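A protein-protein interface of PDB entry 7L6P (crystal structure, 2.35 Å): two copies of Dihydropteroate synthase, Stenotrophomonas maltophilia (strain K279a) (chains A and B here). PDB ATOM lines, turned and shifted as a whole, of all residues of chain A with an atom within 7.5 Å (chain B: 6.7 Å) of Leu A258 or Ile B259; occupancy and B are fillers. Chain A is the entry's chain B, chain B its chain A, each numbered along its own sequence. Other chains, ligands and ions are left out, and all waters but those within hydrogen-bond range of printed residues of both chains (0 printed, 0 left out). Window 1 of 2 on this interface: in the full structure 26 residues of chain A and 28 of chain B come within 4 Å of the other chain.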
ATOM      1  N   LEU A 214     -22.934   2.500 -33.295  1.00  0.00           N
ATOM      2  CA  LEU A 214     -22.447   1.751 -32.138  1.00  0.00           C
ATOM      3  C   LEU A 214     -21.036   1.211 -32.395  1.00  0.00           C
ATOM      4  O   LEU A 214     -20.167   1.305 -31.521  1.00  0.00           O
ATOM      5  CB  LEU A 214     -23.424   0.629 -31.771  1.00  0.00           C
ATOM      6  CG  LEU A 214     -23.005  -0.244 -30.566  1.00  0.00           C
ATOM      7  CD1 LEU A 214     -22.797   0.589 -29.312  1.00  0.00           C
ATOM      8  CD2 LEU A 214     -23.972  -1.383 -30.280  1.00  0.00           C
ATOM      9  N   LEU A 231     -29.662   1.885 -25.486  1.00  0.00           N
ATOM     10  CA  LEU A 231     -30.176   0.968 -26.494  1.00  0.00           C
ATOM     11  C   LEU A 231     -31.199   0.009 -25.914  1.00  0.00           C
ATOM     12  O   LEU A 231     -31.450  -1.046 -26.509  1.00  0.00           O
ATOM     13  CB  LEU A 231     -29.050   0.170 -27.135  1.00  0.00           C
ATOM     14  CG  LEU A 231     -28.022   1.008 -27.876  1.00  0.00           C
ATOM     15  CD1 LEU A 231     -26.723   1.112 -27.055  1.00  0.00           C
ATOM     16  CD2 LEU A 231     -27.773   0.403 -29.251  1.00  0.00           C
ATOM     17  N   ALA A 252     -30.391  -9.052 -25.806  1.00  0.00           N
ATOM     18  CA  ALA A 252     -29.772  -8.179 -26.801  1.00  0.00           C
ATOM     19  C   ALA A 252     -29.438  -6.811 -26.232  1.00  0.00           C
ATOM     20  O   ALA A 252     -28.458  -6.192 -26.651  1.00  0.00           O
ATOM     21  CB  ALA A 252     -30.687  -8.000 -28.015  1.00  0.00           C
ATOM     22  N   SER A 253     -30.228  -6.323 -25.279  1.00  0.00           N
ATOM     23  CA  SER A 253     -29.901  -5.047 -24.656  1.00  0.00           C
ATOM     24  C   SER A 253     -28.645  -5.164 -23.817  1.00  0.00           C
ATOM     25  O   SER A 253     -27.805  -4.255 -23.801  1.00  0.00           O
ATOM     26  CB  SER A 253     -31.072  -4.562 -23.806  1.00  0.00           C
ATOM     27  OG  SER A 253     -32.207  -4.359 -24.617  1.00  0.00           O
ATOM     28  N   VAL A 254     -28.521  -6.264 -23.081  1.00  0.00           N
ATOM     29  CA  VAL A 254     -27.306  -6.493 -22.315  1.00  0.00           C
ATOM     30  C   VAL A 254     -26.098  -6.568 -23.234  1.00  0.00           C
ATOM     31  O   VAL A 254     -25.064  -5.940 -22.978  1.00  0.00           O
ATOM     32  CB  VAL A 254     -27.439  -7.765 -21.472  1.00  0.00           C
ATOM     33  CG1 VAL A 254     -26.017  -8.334 -21.147  1.00  0.00           C
ATOM     34  CG2 VAL A 254     -28.209  -7.435 -20.231  1.00  0.00           C
ATOM     35  N   ALA A 255     -26.212  -7.336 -24.318  1.00  0.00           N
ATOM     36  CA  ALA A 255     -25.118  -7.380 -25.283  1.00  0.00           C
ATOM     37  C   ALA A 255     -24.841  -5.999 -25.857  1.00  0.00           C
ATOM     38  O   ALA A 255     -23.680  -5.617 -26.039  1.00  0.00           O
ATOM     39  CB  ALA A 255     -25.433  -8.363 -26.405  1.00  0.00           C
ATOM     40  N   ALA A 256     -25.891  -5.244 -26.187  1.00  0.00           N
ATOM     41  CA  ALA A 256     -25.680  -3.930 -26.783  1.00  0.00           C
ATOM     42  C   ALA A 256     -24.977  -2.988 -25.811  1.00  0.00           C
ATOM     43  O   ALA A 256     -24.015  -2.301 -26.177  1.00  0.00           O
ATOM     44  CB  ALA A 256     -27.018  -3.338 -27.250  1.00  0.00           C
ATOM     45  N   HIS A 257     -25.426  -2.954 -24.561  1.00  0.00           N
ATOM     46  CA  HIS A 257     -24.839  -2.026 -23.601  1.00  0.00           C
ATOM     47  C   HIS A 257     -23.426  -2.438 -23.216  1.00  0.00           C
ATOM     48  O   HIS A 257     -22.575  -1.573 -22.972  1.00  0.00           O
ATOM     49  CB  HIS A 257     -25.751  -1.919 -22.381  1.00  0.00           C
ATOM     50  CG  HIS A 257     -27.025  -1.185 -22.669  1.00  0.00           C
ATOM     51  ND1 HIS A 257     -28.268  -1.702 -22.383  1.00  0.00           N
ATOM     52  CD2 HIS A 257     -27.243   0.020 -23.252  1.00  0.00           C
ATOM     53  CE1 HIS A 257     -29.195  -0.842 -22.759  1.00  0.00           C
ATOM     54  NE2 HIS A 257     -28.598   0.211 -23.289  1.00  0.00           N
ATOM     55  N   LEU A 258     -23.141  -3.738 -23.179  1.00  0.00           N
ATOM     56  CA  LEU A 258     -21.765  -4.168 -22.963  1.00  0.00           C
ATOM     57  C   LEU A 258     -20.862  -3.633 -24.070  1.00  0.00           C
ATOM     58  O   LEU A 258     -19.811  -3.031 -23.802  1.00  0.00           O
ATOM     59  CB  LEU A 258     -21.698  -5.697 -22.903  1.00  0.00           C
ATOM     60  CG  LEU A 258     -20.294  -6.250 -22.631  1.00  0.00           C
ATOM     61  CD1 LEU A 258     -19.739  -5.569 -21.398  1.00  0.00           C
ATOM     62  CD2 LEU A 258     -20.268  -7.773 -22.453  1.00  0.00           C
ATOM     63  N   ILE A 259     -21.284  -3.809 -25.329  1.00  0.00           N
ATOM     64  CA  ILE A 259     -20.495  -3.321 -26.458  1.00  0.00           C
ATOM     65  C   ILE A 259     -20.359  -1.803 -26.403  1.00  0.00           C
ATOM     66  O   ILE A 259     -19.259  -1.263 -26.562  1.00  0.00           O
ATOM     67  CB  ILE A 259     -21.126  -3.808 -27.768  1.00  0.00           C
ATOM     68  CG1 ILE A 259     -21.149  -5.336 -27.762  1.00  0.00           C
ATOM     69  CG2 ILE A 259     -20.323  -3.315 -28.966  1.00  0.00           C
ATOM     70  CD1 ILE A 259     -22.013  -5.942 -28.822  1.00  0.00           C
ATOM     71  N   ALA A 260     -21.457  -1.094 -26.108  1.00  0.00           N
ATOM     72  CA  ALA A 260     -21.376   0.356 -25.951  1.00  0.00           C
ATOM     73  C   ALA A 260     -20.361   0.739 -24.885  1.00  0.00           C
ATOM     74  O   ALA A 260     -19.547   1.647 -25.088  1.00  0.00           O
ATOM     75  CB  ALA A 260     -22.750   0.928 -25.582  1.00  0.00           C
ATOM     76  N   VAL A 261     -20.351   0.015 -23.760  1.00  0.00           N
ATOM     77  CA  VAL A 261     -19.394   0.326 -22.705  1.00  0.00           C
ATOM     78  C   VAL A 261     -17.973   0.038 -23.160  1.00  0.00           C
ATOM     79  O   VAL A 261     -17.069   0.862 -22.971  1.00  0.00           O
ATOM     80  CB  VAL A 261     -19.748  -0.453 -21.428  1.00  0.00           C
ATOM     81  CG1 VAL A 261     -18.543  -0.480 -20.460  1.00  0.00           C
ATOM     82  CG2 VAL A 261     -20.945   0.185 -20.787  1.00  0.00           C
ATOM     83  N   GLN A 262     -17.758  -1.097 -23.822  1.00  0.00           N
ATOM     84  CA  GLN A 262     -16.420  -1.396 -24.341  1.00  0.00           C
ATOM     85  C   GLN A 262     -15.945  -0.334 -25.312  1.00  0.00           C
ATOM     86  O   GLN A 262     -14.739  -0.099 -25.434  1.00  0.00           O
ATOM     87  CB  GLN A 262     -16.406  -2.765 -25.018  1.00  0.00           C
ATOM     88  CG  GLN A 262     -16.730  -3.883 -24.051  1.00  0.00           C
ATOM     89  CD  GLN A 262     -16.978  -5.179 -24.762  1.00  0.00           C
ATOM     90  OE1 GLN A 262     -17.520  -5.184 -25.864  1.00  0.00           O
ATOM     91  NE2 GLN A 262     -16.606  -6.300 -24.129  1.00  0.00           N
ATOM     92  N   ARG A 263     -16.864   0.347 -25.988  1.00  0.00           N
ATOM     93  CA  ARG A 263     -16.453   1.332 -26.972  1.00  0.00           C
ATOM     94  C   ARG A 263     -16.560   2.754 -26.441  1.00  0.00           C
ATOM     95  O   ARG A 263     -16.518   3.710 -27.216  1.00  0.00           O
ATOM     96  CB  ARG A 263     -17.242   1.113 -28.260  1.00  0.00           C
ATOM     97  CG  ARG A 263     -17.106  -0.356 -28.674  1.00  0.00           C
ATOM     98  CD  ARG A 263     -17.360  -0.635 -30.150  1.00  0.00           C
ATOM     99  NE  ARG A 263     -17.113  -2.043 -30.446  1.00  0.00           N
ATOM    100  CZ  ARG A 263     -16.851  -2.531 -31.651  1.00  0.00           C
ATOM    101  NH1 ARG A 263     -16.829  -1.752 -32.726  1.00  0.00           N
ATOM    102  NH2 ARG A 263     -16.624  -3.838 -31.785  1.00  0.00           N
ATOM    103  N   GLY A 264     -16.692   2.914 -25.126  1.00  0.00           N
ATOM    104  CA  GLY A 264     -16.429   4.184 -24.479  1.00  0.00           C
ATOM    105  C   GLY A 264     -17.603   4.798 -23.770  1.00  0.00           C
ATOM    106  O   GLY A 264     -17.434   5.835 -23.110  1.00  0.00           O
ATOM    107  N   ALA A 265     -18.799   4.245 -23.903  1.00  0.00           N
ATOM    108  CA  ALA A 265     -19.922   4.781 -23.154  1.00  0.00           C
ATOM    109  C   ALA A 265     -19.653   4.573 -21.671  1.00  0.00           C
ATOM    110  O   ALA A 265     -19.306   3.464 -21.240  1.00  0.00           O
ATOM    111  CB  ALA A 265     -21.221   4.096 -23.581  1.00  0.00           C
ATOM    112  N   VAL A 268     -24.948   3.976 -19.073  1.00  0.00           N
ATOM    113  CA  VAL A 268     -25.920   3.267 -19.898  1.00  0.00           C
ATOM    114  C   VAL A 268     -27.310   3.465 -19.301  1.00  0.00           C
ATOM    115  O   VAL A 268     -27.503   3.289 -18.092  1.00  0.00           O
ATOM    116  CB  VAL A 268     -25.584   1.773 -20.043  1.00  0.00           C
ATOM    117  CG1 VAL A 268     -24.363   1.610 -20.918  1.00  0.00           C
ATOM    118  CG2 VAL A 268     -25.366   1.110 -18.664  1.00  0.00           C
ATOM    119  N   THR A 276     -28.191  -5.467 -16.534  1.00  0.00           N
ATOM    120  CA  THR A 276     -27.068  -4.659 -16.986  1.00  0.00           C
ATOM    121  C   THR A 276     -25.980  -4.612 -15.925  1.00  0.00           C
ATOM    122  O   THR A 276     -24.789  -4.695 -16.252  1.00  0.00           O
ATOM    123  CB  THR A 276     -27.541  -3.243 -17.313  1.00  0.00           C
ATOM    124  OG1 THR A 276     -28.690  -3.307 -18.165  1.00  0.00           O
ATOM    125  CG2 THR A 276     -26.450  -2.444 -18.030  1.00  0.00           C
ATOM    126  N   ALA A 279     -23.997  -7.895 -15.901  1.00  0.00           N
ATOM    127  CA  ALA A 279     -23.079  -7.940 -17.029  1.00  0.00           C
ATOM    128  C   ALA A 279     -21.875  -7.048 -16.795  1.00  0.00           C
ATOM    129  O   ALA A 279     -20.747  -7.439 -17.097  1.00  0.00           O
ATOM    130  CB  ALA A 279     -23.796  -7.535 -18.313  1.00  0.00           C
ATOM    131  N   LEU A 280     -22.084  -5.846 -16.262  1.00  0.00           N
ATOM    132  CA  LEU A 280     -20.944  -4.956 -16.064  1.00  0.00           C
ATOM    133  C   LEU A 280     -19.988  -5.506 -15.018  1.00  0.00           C
ATOM    134  O   LEU A 280     -18.784  -5.233 -15.081  1.00  0.00           O
ATOM    135  CB  LEU A 280     -21.406  -3.556 -15.678  1.00  0.00           C
ATOM    136  CG  LEU A 280     -22.078  -2.867 -16.863  1.00  0.00           C
ATOM    137  CD1 LEU A 280     -22.516  -1.436 -16.566  1.00  0.00           C
ATOM    138  CD2 LEU A 280     -21.125  -2.930 -18.080  1.00  0.00           C
ATOM    139  N   LYS A 281     -20.503  -6.273 -14.053  1.00  0.00           N
ATOM    140  CA  LYS A 281     -19.639  -6.882 -13.052  1.00  0.00           C
ATOM    141  C   LYS A 281     -18.722  -7.925 -13.681  1.00  0.00           C
ATOM    142  O   LYS A 281     -17.541  -8.012 -13.332  1.00  0.00           O
ATOM    143  CB  LYS A 281     -20.481  -7.495 -11.927  1.00  0.00           C
ATOM    144  CG  LYS A 281     -21.108  -6.472 -10.991  1.00  0.00           C
ATOM    145  CD  LYS A 281     -20.519  -6.551  -9.600  1.00  0.00           C
ATOM    146  CE  LYS A 281     -20.847  -5.335  -8.743  1.00  0.00           C
ATOM    147  NZ  LYS A 281     -22.273  -4.944  -8.855  1.00  0.00           N
ATOM    148  N   ILE A 282     -19.248  -8.729 -14.607  1.00  0.00           N
ATOM    149  CA  ILE A 282     -18.399  -9.656 -15.336  1.00  0.00           C
ATOM    150  C   ILE A 282     -17.332  -8.885 -16.103  1.00  0.00           C
ATOM    151  O   ILE A 282     -16.143  -9.233 -16.065  1.00  0.00           O
ATOM    152  CB  ILE A 282     -19.241 -10.520 -16.287  1.00  0.00           C
ATOM    153  CG1 ILE A 282     -20.376 -11.214 -15.525  1.00  0.00           C
ATOM    154  CG2 ILE A 282     -18.324 -11.518 -17.036  1.00  0.00           C
ATOM    155  CD1 ILE A 282     -19.943 -12.003 -14.314  1.00  0.00           C
ATOM    156  N   TRP A 283     -17.745  -7.810 -16.788  1.00  0.00           N
ATOM    157  CA  TRP A 283     -16.827  -6.987 -17.572  1.00  0.00           C
ATOM    158  C   TRP A 283     -15.757  -6.351 -16.696  1.00  0.00           C
ATOM    159  O   TRP A 283     -14.575  -6.369 -17.047  1.00  0.00           O
ATOM    160  CB  TRP A 283     -17.587  -5.904 -18.355  1.00  0.00           C
ATOM    161  CG  TRP A 283     -16.675  -4.953 -19.103  1.00  0.00           C
ATOM    162  CD1 TRP A 283     -16.583  -3.601 -18.933  1.00  0.00           C
ATOM    163  CD2 TRP A 283     -15.721  -5.285 -20.153  1.00  0.00           C
ATOM    164  NE1 TRP A 283     -15.642  -3.070 -19.802  1.00  0.00           N
ATOM    165  CE2 TRP A 283     -15.103  -4.081 -20.555  1.00  0.00           C
ATOM    166  CE3 TRP A 283     -15.334  -6.480 -20.774  1.00  0.00           C
ATOM    167  CZ2 TRP A 283     -14.122  -4.036 -21.557  1.00  0.00           C
ATOM    168  CZ3 TRP A 283     -14.336  -6.437 -21.766  1.00  0.00           C
ATOM    169  CH2 TRP A 283     -13.744  -5.225 -22.140  1.00  0.00           C
ATOM    170  N   GLN A 284     -16.150  -5.738 -15.580  1.00  0.00           N
ATOM    171  CA  GLN A 284     -15.153  -5.104 -14.718  1.00  0.00           C
ATOM    172  C   GLN A 284     -14.135  -6.127 -14.207  1.00  0.00           C
ATOM    173  O   GLN A 284     -12.935  -5.834 -14.111  1.00  0.00           O
ATOM    174  CB  GLN A 284     -15.827  -4.396 -13.537  1.00  0.00           C
ATOM    175  CG  GLN A 284     -16.622  -3.130 -13.923  1.00  0.00           C
ATOM    176  CD  GLN A 284     -17.801  -2.839 -12.955  1.00  0.00           C
ATOM    177  OE1 GLN A 284     -17.887  -3.425 -11.863  1.00  0.00           O
ATOM    178  NE2 GLN A 284     -18.693  -1.915 -13.351  1.00  0.00           N
ATOM    179  N   VAL A 286     -13.226  -8.862 -15.761  1.00  0.00           N
ATOM    180  CA  VAL A 286     -12.358  -9.201 -16.882  1.00  0.00           C
ATOM    181  C   VAL A 286     -11.338  -8.092 -17.123  1.00  0.00           C
ATOM    182  O   VAL A 286     -10.149  -8.366 -17.341  1.00  0.00           O
ATOM    183  CB  VAL A 286     -13.202  -9.506 -18.132  1.00  0.00           C
ATOM    184  CG1 VAL A 286     -12.309  -9.579 -19.380  1.00  0.00           C
ATOM    185  CG2 VAL A 286     -13.942 -10.824 -17.925  1.00  0.00           C
ATOM    186  N   GLU A 287     -11.773  -6.829 -17.028  1.00  0.00           N
ATOM    187  CA  GLU A 287     -10.883  -5.703 -17.302  1.00  0.00           C
ATOM    188  C   GLU A 287      -9.823  -5.537 -16.233  1.00  0.00           C
ATOM    189  O   GLU A 287      -8.748  -5.001 -16.513  1.00  0.00           O
ATOM    190  CB  GLU A 287     -11.682  -4.409 -17.411  1.00  0.00           C
ATOM    191  CG  GLU A 287     -12.389  -4.236 -18.705  1.00  0.00           C
ATOM    192  CD  GLU A 287     -11.439  -3.846 -19.839  1.00  0.00           C
ATOM    193  OE1 GLU A 287     -10.705  -4.729 -20.379  1.00  0.00           O
ATOM    194  OE2 GLU A 287     -11.441  -2.634 -20.182  1.00  0.00           O
ATOM    195  N   LEU B 214     -10.250 -16.187 -18.709  1.00  0.00           N
ATOM    196  CA  LEU B 214     -11.173 -15.586 -19.669  1.00  0.00           C
ATOM    197  C   LEU B 214     -10.570 -14.336 -20.275  1.00  0.00           C
ATOM    198  O   LEU B 214     -10.639 -14.135 -21.489  1.00  0.00           O
ATOM    199  CB  LEU B 214     -12.515 -15.257 -19.010  1.00  0.00           C
ATOM    200  CG  LEU B 214     -13.547 -14.562 -19.929  1.00  0.00           C
ATOM    201  CD1 LEU B 214     -13.845 -15.412 -21.166  1.00  0.00           C
ATOM    202  CD2 LEU B 214     -14.858 -14.183 -19.167  1.00  0.00           C
ATOM    203  N   ALA B 215      -9.929 -13.507 -19.450  1.00  0.00           N
ATOM    204  CA  ALA B 215      -9.376 -12.253 -19.947  1.00  0.00           C
ATOM    205  C   ALA B 215      -8.230 -12.489 -20.930  1.00  0.00           C
ATOM    206  O   ALA B 215      -8.125 -11.779 -21.937  1.00  0.00           O
ATOM    207  CB  ALA B 215      -8.912 -11.390 -18.779  1.00  0.00           C
ATOM    208  N   SER B 217      -7.745 -15.341 -22.627  1.00  0.00           N
ATOM    209  CA  SER B 217      -8.019 -16.552 -23.404  1.00  0.00           C
ATOM    210  C   SER B 217      -7.558 -16.455 -24.858  1.00  0.00           C
ATOM    211  O   SER B 217      -7.335 -17.491 -25.499  1.00  0.00           O
ATOM    212  CB  SER B 217      -9.507 -16.882 -23.381  1.00  0.00           C
ATOM    213  OG  SER B 217     -10.270 -15.820 -23.892  1.00  0.00           O
ATOM    214  N   VAL B 254     -24.709 -14.499 -20.462  1.00  0.00           N
ATOM    215  CA  VAL B 254     -24.678 -13.840 -21.756  1.00  0.00           C
ATOM    216  C   VAL B 254     -23.446 -12.951 -21.857  1.00  0.00           C
ATOM    217  O   VAL B 254     -22.706 -12.997 -22.849  1.00  0.00           O
ATOM    218  CB  VAL B 254     -25.987 -13.052 -21.964  1.00  0.00           C
ATOM    219  CG1 VAL B 254     -25.847 -11.978 -23.061  1.00  0.00           C
ATOM    220  CG2 VAL B 254     -27.168 -14.009 -22.227  1.00  0.00           C
ATOM    221  N   ALA B 255     -23.186 -12.147 -20.820  1.00  0.00           N
ATOM    222  CA  ALA B 255     -21.997 -11.296 -20.839  1.00  0.00           C
ATOM    223  C   ALA B 255     -20.718 -12.135 -20.903  1.00  0.00           C
ATOM    224  O   ALA B 255     -19.805 -11.861 -21.701  1.00  0.00           O
ATOM    225  CB  ALA B 255     -21.992 -10.382 -19.620  1.00  0.00           C
ATOM    226  N   ALA B 256     -20.648 -13.190 -20.097  1.00  0.00           N
ATOM    227  CA  ALA B 256     -19.430 -13.985 -20.080  1.00  0.00           C
ATOM    228  C   ALA B 256     -19.188 -14.608 -21.440  1.00  0.00           C
ATOM    229  O   ALA B 256     -18.063 -14.582 -21.957  1.00  0.00           O
ATOM    230  CB  ALA B 256     -19.510 -15.049 -18.985  1.00  0.00           C
ATOM    231  N   HIS B 257     -20.239 -15.150 -22.054  1.00  0.00           N
ATOM    232  CA  HIS B 257     -20.046 -15.826 -23.334  1.00  0.00           C
ATOM    233  C   HIS B 257     -19.756 -14.850 -24.470  1.00  0.00           C
ATOM    234  O   HIS B 257     -18.982 -15.178 -25.371  1.00  0.00           O
ATOM    235  CB  HIS B 257     -21.264 -16.693 -23.640  1.00  0.00           C
ATOM    236  CG  HIS B 257     -21.339 -17.896 -22.766  1.00  0.00           C
ATOM    237  ND1 HIS B 257     -22.462 -18.231 -22.042  1.00  0.00           N
ATOM    238  CD2 HIS B 257     -20.398 -18.828 -22.462  1.00  0.00           C
ATOM    239  CE1 HIS B 257     -22.213 -19.319 -21.329  1.00  0.00           C
ATOM    240  NE2 HIS B 257     -20.968 -19.696 -21.561  1.00  0.00           N
ATOM    241  N   LEU B 258     -20.337 -13.652 -24.446  1.00  0.00           N
ATOM    242  CA  LEU B 258     -19.971 -12.636 -25.431  1.00  0.00           C
ATOM    243  C   LEU B 258     -18.493 -12.298 -25.332  1.00  0.00           C
ATOM    244  O   LEU B 258     -17.788 -12.217 -26.348  1.00  0.00           O
ATOM    245  CB  LEU B 258     -20.831 -11.377 -25.243  1.00  0.00           C
ATOM    246  CG  LEU B 258     -20.563 -10.167 -26.126  1.00  0.00           C
ATOM    247  CD1 LEU B 258     -20.472 -10.558 -27.595  1.00  0.00           C
ATOM    248  CD2 LEU B 258     -21.709  -9.167 -25.933  1.00  0.00           C
ATOM    249  N   ILE B 259     -18.011 -12.076 -24.105  1.00  0.00           N
ATOM    250  CA  ILE B 259     -16.600 -11.771 -23.893  1.00  0.00           C
ATOM    251  C   ILE B 259     -15.731 -12.927 -24.351  1.00  0.00           C
ATOM    252  O   ILE B 259     -14.673 -12.724 -24.951  1.00  0.00           O
ATOM    253  CB  ILE B 259     -16.340 -11.442 -22.412  1.00  0.00           C
ATOM    254  CG1 ILE B 259     -17.131 -10.196 -21.991  1.00  0.00           C
ATOM    255  CG2 ILE B 259     -14.832 -11.328 -22.125  1.00  0.00           C
ATOM    256  CD1 ILE B 259     -17.159  -9.981 -20.479  1.00  0.00           C
ATOM    257  N   ALA B 260     -16.137 -14.154 -24.032  1.00  0.00           N
ATOM    258  CA  ALA B 260     -15.378 -15.323 -24.468  1.00  0.00           C
ATOM    259  C   ALA B 260     -15.278 -15.372 -25.984  1.00  0.00           C
ATOM    260  O   ALA B 260     -14.235 -15.747 -26.535  1.00  0.00           O
ATOM    261  CB  ALA B 260     -16.023 -16.600 -23.927  1.00  0.00           C
ATOM    262  N   VAL B 261     -16.365 -15.027 -26.682  1.00  0.00           N
ATOM    263  CA  VAL B 261     -16.345 -15.039 -28.142  1.00  0.00           C
ATOM    264  C   VAL B 261     -15.481 -13.905 -28.676  1.00  0.00           C
ATOM    265  O   VAL B 261     -14.713 -14.077 -29.635  1.00  0.00           O
ATOM    266  CB  VAL B 261     -17.777 -14.996 -28.680  1.00  0.00           C
ATOM    267  CG1 VAL B 261     -17.794 -14.673 -30.201  1.00  0.00           C
ATOM    268  CG2 VAL B 261     -18.447 -16.307 -28.383  1.00  0.00           C
ATOM    269  N   GLN B 262     -15.572 -12.729 -28.065  1.00  0.00           N
ATOM    270  CA  GLN B 262     -14.704 -11.639 -28.492  1.00  0.00           C
ATOM    271  C   GLN B 262     -13.228 -11.999 -28.363  1.00  0.00           C
ATOM    272  O   GLN B 262     -12.391 -11.431 -29.067  1.00  0.00           O
ATOM    273  CB  GLN B 262     -14.996 -10.381 -27.686  1.00  0.00           C
ATOM    274  CG  GLN B 262     -16.409  -9.849 -27.875  1.00  0.00           C
ATOM    275  CD  GLN B 262     -16.726  -8.716 -26.944  1.00  0.00           C
ATOM    276  OE1 GLN B 262     -16.282  -8.695 -25.794  1.00  0.00           O
ATOM    277  NE2 GLN B 262     -17.481  -7.740 -27.442  1.00  0.00           N
ATOM    278  N   ARG B 263     -12.880 -12.895 -27.447  1.00  0.00           N
ATOM    279  CA  ARG B 263     -11.489 -13.239 -27.216  1.00  0.00           C
ATOM    280  C   ARG B 263     -11.111 -14.585 -27.820  1.00  0.00           C
ATOM    281  O   ARG B 263     -10.053 -15.128 -27.495  1.00  0.00           O
ATOM    282  CB  ARG B 263     -11.186 -13.174 -25.720  1.00  0.00           C
ATOM    283  CG  ARG B 263     -11.638 -11.833 -25.173  1.00  0.00           C
ATOM    284  CD  ARG B 263     -10.981 -11.372 -23.886  1.00  0.00           C
ATOM    285  NE  ARG B 263     -11.469 -10.029 -23.581  1.00  0.00           N
ATOM    286  CZ  ARG B 263     -10.802  -9.137 -22.866  1.00  0.00           C
ATOM    287  NH1 ARG B 263      -9.633  -9.428 -22.312  1.00  0.00           N
ATOM    288  NH2 ARG B 263     -11.285  -7.903 -22.763  1.00  0.00           N
ATOM    289  N   GLY B 264     -11.936 -15.115 -28.714  1.00  0.00           N
ATOM    290  CA  GLY B 264     -11.535 -16.164 -29.630  1.00  0.00           C
ATOM    291  C   GLY B 264     -12.325 -17.447 -29.554  1.00  0.00           C
ATOM    292  O   GLY B 264     -12.102 -18.327 -30.398  1.00  0.00           O
ATOM    293  N   ALA B 265     -13.221 -17.615 -28.580  1.00  0.00           N
ATOM    294  CA  ALA B 265     -14.040 -18.819 -28.519  1.00  0.00           C
ATOM    295  C   ALA B 265     -14.952 -18.880 -29.731  1.00  0.00           C
ATOM    296  O   ALA B 265     -15.618 -17.890 -30.069  1.00  0.00           O
ATOM    297  CB  ALA B 265     -14.879 -18.819 -27.248  1.00  0.00           C
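OG of Ser B217 lies within hydrogen-bond range of O of Leu B214 (3.0 Å).
O of Ala B215 lies within hydrogen-bond range of NH1 of Arg B263, at 2.8 Å.
Among the printed residues, pairs that only touch across the chains: Trp A283 with Arg B263 (3.5 Å), Val A286 with Ala B215 (3.6 Å), Ala A279 with Ala B255 (3.6 Å), Val A286 with Leu B214 (3.7 Å), Val A286 with Arg B263 (3.8 Å), Ala A255 with Leu B258 (3.8 Å), Ile A282 with Ile B259 (3.9 Å), Trp A283 with Ile B259 (3.96 Å) and Leu A258 with Ile B259 (3.99 Å).
NE2 of Gln A262 is in hydrogen-bond range of OE1 of Gln B262 (2.9 Å).
Of the 15 printed residues of chain B, 7 touch a printed residue of chain A.
Printed residues of chain B that touch a printed residue of chain A: Leu B214, Ala B215, Ala B255, Leu B258, Ile B259, Gln B262 and Arg B263.
Hydrophobic or aromatic side chains of chain A that line the printed part of chain B: Ala A255, Leu A258, Ala A279, Ile A282, Trp A283 and Val A286.
Among the printed residues, 10 pairs touch across the chains.
Among the printed residues, no Asp or Glu carboxylate lies within 4 Å of a Lys or Arg side-chain nitrogen of the other chain.
Of the printed residues of chain B, Val A286 touches Leu B214, Ala B215 and Arg B263.
Of the printed residues of chain A, Gln B262 touches Gln A262.
Printed residues of chain B within 4 Å of Ala A279: Ala B255.
Of the printed residues of chain B, Gln A262 touches Gln B262.
The nearest printed residue of chain B that does not touch Leu A258 is Leu B258 (4.02 Å).
Ala A255 touches Leu B258, but with the chains exchanged Leu A258 does not touch Ala B255 (4.2 Å).
Leu A258 touches Ile B259, but with the chains exchanged Ile A259 does not touch Leu B258 (4.3 Å).
Gln B262 touches its own counterpart, Gln A262.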
